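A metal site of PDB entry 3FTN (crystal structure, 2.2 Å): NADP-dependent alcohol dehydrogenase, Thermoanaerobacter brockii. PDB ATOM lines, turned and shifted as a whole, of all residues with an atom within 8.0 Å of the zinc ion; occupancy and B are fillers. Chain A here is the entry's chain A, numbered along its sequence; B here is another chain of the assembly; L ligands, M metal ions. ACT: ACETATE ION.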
ATOM      1  N   ALA A  35       3.202  18.620  16.375  1.00  0.00           N
ATOM      2  CA  ALA A  35       2.072  19.540  16.467  1.00  0.00           C
ATOM      3  C   ALA A  35       2.439  20.760  17.334  1.00  0.00           C
ATOM      4  O   ALA A  35       3.277  20.643  18.241  1.00  0.00           O
ATOM      5  CB  ALA A  35       0.845  18.823  17.027  1.00  0.00           C
ATOM      6  N   PRO A  36       1.829  21.922  17.062  1.00  0.00           N
ATOM      7  CA  PRO A  36       2.065  23.049  17.970  1.00  0.00           C
ATOM      8  C   PRO A  36       0.997  23.079  19.045  1.00  0.00           C
ATOM      9  O   PRO A  36      -0.081  22.482  18.887  1.00  0.00           O
ATOM     10  CB  PRO A  36       1.902  24.270  17.060  1.00  0.00           C
ATOM     11  CG  PRO A  36       1.184  23.748  15.800  1.00  0.00           C
ATOM     12  CD  PRO A  36       0.928  22.290  15.971  1.00  0.00           C
ATOM     13  N   CYS A  37       1.283  23.799  20.122  1.00  0.00           N
ATOM     14  CA  CYS A  37       0.410  23.875  21.276  1.00  0.00           C
ATOM     15  C   CYS A  37       0.111  25.343  21.573  1.00  0.00           C
ATOM     16  O   CYS A  37       0.992  26.199  21.435  1.00  0.00           O
ATOM     17  CB  CYS A  37       1.069  23.233  22.507  1.00  0.00           C
ATOM     18  SG  CYS A  37       0.013  23.207  24.012  1.00  0.00           S
ATOM     19  N   THR A  38      -1.118  25.609  21.982  1.00  0.00           N
ATOM     20  CA  THR A  38      -1.518  26.935  22.476  1.00  0.00           C
ATOM     21  C   THR A  38      -0.594  27.426  23.574  1.00  0.00           C
ATOM     22  O   THR A  38      -0.356  28.634  23.690  1.00  0.00           O
ATOM     23  CB  THR A  38      -2.937  26.922  23.042  1.00  0.00           C
ATOM     24  OG1 THR A  38      -3.013  25.996  24.136  1.00  0.00           O
ATOM     25  CG2 THR A  38      -3.934  26.500  21.974  1.00  0.00           C
ATOM     26  N   SER A  39      -0.062  26.513  24.386  1.00  0.00           N
ATOM     27  CA  SER A  39       0.862  26.908  25.449  1.00  0.00           C
ATOM     28  C   SER A  39       2.055  27.668  24.887  1.00  0.00           C
ATOM     29  O   SER A  39       2.475  28.654  25.465  1.00  0.00           O
ATOM     30  CB  SER A  39       1.352  25.706  26.255  1.00  0.00           C
ATOM     31  OG  SER A  39       2.291  24.946  25.496  1.00  0.00           O
ATOM     32  N   ASP A  40       2.602  27.226  23.756  1.00  0.00           N
ATOM     33  CA  ASP A  40       3.719  27.971  23.187  1.00  0.00           C
ATOM     34  C   ASP A  40       3.282  29.377  22.751  1.00  0.00           C
ATOM     35  O   ASP A  40       4.104  30.296  22.676  1.00  0.00           O
ATOM     36  CB  ASP A  40       4.387  27.214  22.034  1.00  0.00           C
ATOM     37  CG  ASP A  40       5.337  26.142  22.518  1.00  0.00           C
ATOM     38  OD1 ASP A  40       5.521  26.055  23.755  1.00  0.00           O
ATOM     39  OD2 ASP A  40       5.895  25.398  21.677  1.00  0.00           O
ATOM     40  N   GLY A  58       7.939  23.807  20.643  1.00  0.00           N
ATOM     41  CA  GLY A  58       7.299  22.518  20.397  1.00  0.00           C
ATOM     42  C   GLY A  58       7.610  21.442  21.424  1.00  0.00           C
ATOM     43  O   GLY A  58       8.772  21.236  21.815  1.00  0.00           O
ATOM     44  N   HIS A  59       6.578  20.725  21.846  1.00  0.00           N
ATOM     45  CA  HIS A  59       6.750  19.617  22.789  1.00  0.00           C
ATOM     46  C   HIS A  59       5.789  18.462  22.488  1.00  0.00           C
ATOM     47  O   HIS A  59       5.491  17.656  23.368  1.00  0.00           O
ATOM     48  CB  HIS A  59       6.564  20.078  24.229  1.00  0.00           C
ATOM     49  CG  HIS A  59       5.356  20.927  24.436  1.00  0.00           C
ATOM     50  ND1 HIS A  59       5.424  22.302  24.532  1.00  0.00           N
ATOM     51  CD2 HIS A  59       4.052  20.605  24.560  1.00  0.00           C
ATOM     52  CE1 HIS A  59       4.210  22.792  24.709  1.00  0.00           C
ATOM     53  NE2 HIS A  59       3.352  21.782  24.724  1.00  0.00           N
ATOM     54  N   GLU A  60       5.330  18.373  21.257  1.00  0.00           N
ATOM     55  CA  GLU A  60       4.496  17.248  20.834  1.00  0.00           C
ATOM     56  C   GLU A  60       5.072  16.580  19.583  1.00  0.00           C
ATOM     57  O   GLU A  60       5.014  17.143  18.495  1.00  0.00           O
ATOM     58  CB  GLU A  60       3.068  17.711  20.548  1.00  0.00           C
ATOM     59  CG  GLU A  60       2.307  18.206  21.776  1.00  0.00           C
ATOM     60  CD  GLU A  60       1.165  19.096  21.381  1.00  0.00           C
ATOM     61  OE1 GLU A  60       0.020  18.588  21.270  1.00  0.00           O
ATOM     62  OE2 GLU A  60       1.424  20.288  21.113  1.00  0.00           O
ATOM     63  N   ALA A  85       5.161  14.948  26.297  1.00  0.00           N
ATOM     64  CA  ALA A  85       5.496  16.373  26.469  1.00  0.00           C
ATOM     65  C   ALA A  85       6.292  16.585  27.753  1.00  0.00           C
ATOM     66  O   ALA A  85       7.178  17.423  27.813  1.00  0.00           O
ATOM     67  CB  ALA A  85       4.225  17.230  26.513  1.00  0.00           C
ATOM     68  N   ILE A  86       5.930  15.830  28.780  1.00  0.00           N
ATOM     69  CA  ILE A  86       6.583  15.917  30.077  1.00  0.00           C
ATOM     70  C   ILE A  86       7.601  14.783  30.212  1.00  0.00           C
ATOM     71  O   ILE A  86       7.249  13.606  30.209  1.00  0.00           O
ATOM     72  CB  ILE A  86       5.538  15.906  31.213  1.00  0.00           C
ATOM     73  CG1 ILE A  86       5.041  17.324  31.484  1.00  0.00           C
ATOM     74  CG2 ILE A  86       6.115  15.328  32.494  1.00  0.00           C
ATOM     75  CD1 ILE A  86       4.396  17.985  30.292  1.00  0.00           C
ATOM     76  N   TRP A 110       8.083  19.364  32.861  1.00  0.00           N
ATOM     77  CA  TRP A 110       7.860  19.833  31.501  1.00  0.00           C
ATOM     78  C   TRP A 110       9.117  20.552  31.016  1.00  0.00           C
ATOM     79  O   TRP A 110       9.415  21.674  31.431  1.00  0.00           O
ATOM     80  CB  TRP A 110       6.612  20.739  31.458  1.00  0.00           C
ATOM     81  CG  TRP A 110       6.499  21.634  30.243  1.00  0.00           C
ATOM     82  CD1 TRP A 110       6.986  21.389  28.987  1.00  0.00           C
ATOM     83  CD2 TRP A 110       5.822  22.901  30.169  1.00  0.00           C
ATOM     84  NE1 TRP A 110       6.675  22.437  28.150  1.00  0.00           N
ATOM     85  CE2 TRP A 110       5.963  23.373  28.856  1.00  0.00           C
ATOM     86  CE3 TRP A 110       5.153  23.697  31.110  1.00  0.00           C
ATOM     87  CZ2 TRP A 110       5.453  24.613  28.440  1.00  0.00           C
ATOM     88  CZ3 TRP A 110       4.637  24.930  30.704  1.00  0.00           C
ATOM     89  CH2 TRP A 110       4.796  25.367  29.379  1.00  0.00           C
ATOM     90  N   PHE A 112      10.667  20.339  27.313  1.00  0.00           N
ATOM     91  CA  PHE A 112      10.613  20.836  25.940  1.00  0.00           C
ATOM     92  C   PHE A 112       9.839  22.159  25.864  1.00  0.00           C
ATOM     93  O   PHE A 112       8.690  22.218  26.289  1.00  0.00           O
ATOM     94  CB  PHE A 112       9.908  19.841  25.010  1.00  0.00           C
ATOM     95  CG  PHE A 112      10.653  18.550  24.779  1.00  0.00           C
ATOM     96  CD1 PHE A 112      11.978  18.541  24.369  1.00  0.00           C
ATOM     97  CD2 PHE A 112       9.997  17.334  24.938  1.00  0.00           C
ATOM     98  CE1 PHE A 112      12.641  17.332  24.134  1.00  0.00           C
ATOM     99  CE2 PHE A 112      10.670  16.118  24.696  1.00  0.00           C
ATOM    100  CZ  PHE A 112      11.977  16.120  24.291  1.00  0.00           C
ATOM    101  N   SER A 113      10.461  23.193  25.303  1.00  0.00           N
ATOM    102  CA  SER A 113       9.872  24.515  25.129  1.00  0.00           C
ATOM    103  C   SER A 113       9.505  25.208  26.444  1.00  0.00           C
ATOM    104  O   SER A 113       8.818  26.232  26.432  1.00  0.00           O
ATOM    105  CB  SER A 113       8.690  24.497  24.120  1.00  0.00           C
ATOM    106  OG  SER A 113       7.438  24.241  24.740  1.00  0.00           O
ATOM    107  N   PRO A 149       1.018  12.828  23.297  1.00  0.00           N
ATOM    108  CA  PRO A 149       2.019  13.407  24.216  1.00  0.00           C
ATOM    109  C   PRO A 149       1.504  14.505  25.124  1.00  0.00           C
ATOM    110  O   PRO A 149       2.159  14.827  26.114  1.00  0.00           O
ATOM    111  CB  PRO A 149       3.048  14.002  23.252  1.00  0.00           C
ATOM    112  CG  PRO A 149       2.986  13.072  22.066  1.00  0.00           C
ATOM    113  CD  PRO A 149       1.505  12.802  21.912  1.00  0.00           C
ATOM    114  N   ASP A 150       0.354  15.092  24.791  1.00  0.00           N
ATOM    115  CA  ASP A 150      -0.036  16.336  25.454  1.00  0.00           C
ATOM    116  C   ASP A 150      -1.554  16.502  25.505  1.00  0.00           C
ATOM    117  O   ASP A 150      -2.151  16.538  26.578  1.00  0.00           O
ATOM    118  CB  ASP A 150       0.630  17.514  24.740  1.00  0.00           C
ATOM    119  CG  ASP A 150       0.344  18.860  25.399  1.00  0.00           C
ATOM    120  OD1 ASP A 150      -0.539  18.973  26.278  1.00  0.00           O
ATOM    121  OD2 ASP A 150       1.023  19.831  25.000  1.00  0.00           O
ATOM    122  N   MET A 151      -2.172  16.569  24.329  1.00  0.00           N
ATOM    123  CA  MET A 151      -3.624  16.743  24.264  1.00  0.00           C
ATOM    124  C   MET A 151      -4.363  15.687  25.080  1.00  0.00           C
ATOM    125  O   MET A 151      -5.191  16.032  25.926  1.00  0.00           O
ATOM    126  CB  MET A 151      -4.114  16.777  22.803  1.00  0.00           C
ATOM    127  CG  MET A 151      -3.486  17.894  21.952  1.00  0.00           C
ATOM    128  SD  MET A 151      -3.826  19.561  22.609  1.00  0.00           S
ATOM    129  CE  MET A 151      -2.387  19.830  23.669  1.00  0.00           C
ATOM    130  N   THR A 154      -3.277  15.558  28.927  1.00  0.00           N
ATOM    131  CA  THR A 154      -3.770  16.770  29.603  1.00  0.00           C
ATOM    132  C   THR A 154      -5.298  16.715  29.824  1.00  0.00           C
ATOM    133  O   THR A 154      -5.778  16.842  30.968  1.00  0.00           O
ATOM    134  CB  THR A 154      -3.373  18.038  28.808  1.00  0.00           C
ATOM    135  OG1 THR A 154      -1.947  18.146  28.758  1.00  0.00           O
ATOM    136  CG2 THR A 154      -3.940  19.314  29.453  1.00  0.00           C
ATOM    137  N   VAL A 178      -7.740  20.287  24.105  1.00  0.00           N
ATOM    138  CA  VAL A 178      -7.673  19.818  25.485  1.00  0.00           C
ATOM    139  C   VAL A 178      -9.052  19.542  26.102  1.00  0.00           C
ATOM    140  O   VAL A 178      -9.287  18.486  26.707  1.00  0.00           O
ATOM    141  CB  VAL A 178      -6.837  20.788  26.344  1.00  0.00           C
ATOM    142  CG1 VAL A 178      -7.025  20.488  27.826  1.00  0.00           C
ATOM    143  CG2 VAL A 178      -5.364  20.670  25.941  1.00  0.00           C
ATOM    144  N   TYR A 267      -4.068  26.397  30.960  1.00  0.00           N
ATOM    145  CA  TYR A 267      -2.829  27.106  31.201  1.00  0.00           C
ATOM    146  C   TYR A 267      -3.083  28.602  31.111  1.00  0.00           C
ATOM    147  O   TYR A 267      -3.069  29.195  30.037  1.00  0.00           O
ATOM    148  CB  TYR A 267      -1.781  26.639  30.169  1.00  0.00           C
ATOM    149  CG  TYR A 267      -0.492  27.431  30.136  1.00  0.00           C
ATOM    150  CD1 TYR A 267      -0.046  28.143  31.256  1.00  0.00           C
ATOM    151  CD2 TYR A 267       0.296  27.440  28.998  1.00  0.00           C
ATOM    152  CE1 TYR A 267       1.142  28.854  31.214  1.00  0.00           C
ATOM    153  CE2 TYR A 267       1.494  28.145  28.948  1.00  0.00           C
ATOM    154  CZ  TYR A 267       1.914  28.847  30.056  1.00  0.00           C
ATOM    155  OH  TYR A 267       3.085  29.544  30.003  1.00  0.00           O
ATOM    156  N   LEU A 294      -0.494  20.029  35.934  1.00  0.00           N
ATOM    157  CA  LEU A 294       0.225  19.756  34.714  1.00  0.00           C
ATOM    158  C   LEU A 294       0.034  18.266  34.366  1.00  0.00           C
ATOM    159  O   LEU A 294      -0.007  17.404  35.259  1.00  0.00           O
ATOM    160  CB  LEU A 294       1.718  20.049  34.927  1.00  0.00           C
ATOM    161  CG  LEU A 294       2.652  19.817  33.737  1.00  0.00           C
ATOM    162  CD1 LEU A 294       2.257  20.731  32.575  1.00  0.00           C
ATOM    163  CD2 LEU A 294       4.098  20.078  34.175  1.00  0.00           C
ATOM    164  N   CYS A 295      -0.083  17.973  33.082  1.00  0.00           N
ATOM    165  CA  CYS A 295      -0.331  16.609  32.624  1.00  0.00           C
ATOM    166  C   CYS A 295       0.807  15.662  32.998  1.00  0.00           C
ATOM    167  O   CYS A 295       1.974  16.049  32.968  1.00  0.00           O
ATOM    168  CB  CYS A 295      -0.509  16.572  31.103  1.00  0.00           C
ATOM    169  SG  CYS A 295       0.899  17.179  30.145  1.00  0.00           S
ATOM    170  N   LYS A 346      -6.618  21.047  15.930  1.00  0.00           N
ATOM    171  CA  LYS A 346      -5.187  20.821  16.062  1.00  0.00           C
ATOM    172  C   LYS A 346      -4.542  20.599  14.680  1.00  0.00           C
ATOM    173  O   LYS A 346      -5.083  19.855  13.850  1.00  0.00           O
ATOM    174  CB  LYS A 346      -4.946  19.651  17.014  1.00  0.00           C
ATOM    175  CG  LYS A 346      -3.548  19.548  17.592  1.00  0.00           C
ATOM    176  CD  LYS A 346      -3.330  20.429  18.847  1.00  0.00           C
ATOM    177  CE  LYS A 346      -1.939  20.128  19.386  1.00  0.00           C
ATOM    178  NZ  LYS A 346      -1.571  20.884  20.601  1.00  0.00           N
ATOM    179  N   MET B 285      -1.349  24.739  37.230  1.00  0.00           N
ATOM    180  CA  MET B 285      -0.785  23.430  36.928  1.00  0.00           C
ATOM    181  C   MET B 285       0.171  22.878  37.998  1.00  0.00           C
ATOM    182  O   MET B 285       0.802  21.853  37.788  1.00  0.00           O
ATOM    183  CB  MET B 285      -0.079  23.453  35.573  1.00  0.00           C
ATOM    184  CG  MET B 285      -1.060  23.637  34.380  1.00  0.00           C
ATOM    185  SD  MET B 285      -0.207  23.877  32.801  1.00  0.00           S
ATOM    186  CE  MET B 285       0.943  25.181  33.253  1.00  0.00           C
HETATM  187  C   ACT L   1       1.413  22.129  28.670  1.00  0.00           C
HETATM  188  O   ACT L   1       0.986  21.648  29.732  1.00  0.00           O
HETATM  189  OXT ACT L   1       0.882  21.696  27.633  1.00  0.00           O
HETATM  190  CH3 ACT L   1       2.487  23.163  28.638  1.00  0.00           C
HETATM  191 ZN    ZN M   1       1.325  21.805  25.379  1.00  0.00          ZN
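The backbone carbonyl oxygen of Asp 150 sits at hydrogen-bond distance from the side-chain hydroxyl of Thr 154, 2.7 Å away.
NE2 of His 59 sits close to OG of Ser 39.
A ring nitrogen (ND1) of His 59 is in hydrogen-bond range of the side-chain hydroxyl (OG) of Ser 113, 2.8 Å away.
The side-chain sulfur (SG) of Cys 37 sits close to the side-chain hydroxyl (OG) of Ser 39 (3.2 Å).
Ser 39 touches the zinc ion (OG to ZN, 3.3 Å).
Within 4 Å of the zinc ion: Cys 37, Ser 39, His 59 and Asp 150.
The nearest printed residue that does not touch the zinc ion is Glu 60 (4.5 Å).
The zinc ion is bound by the side-chain carboxylate (OD2) of Asp 150 (2.0 Å), a ring nitrogen (NE2) of His 59 (2.1 Å), an oxygen (OXT) of the ligand (2.3 Å) and the side-chain sulfur (SG) of Cys 37 (2.4 Å).
The zinc ion has four donor atoms within binding distance.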
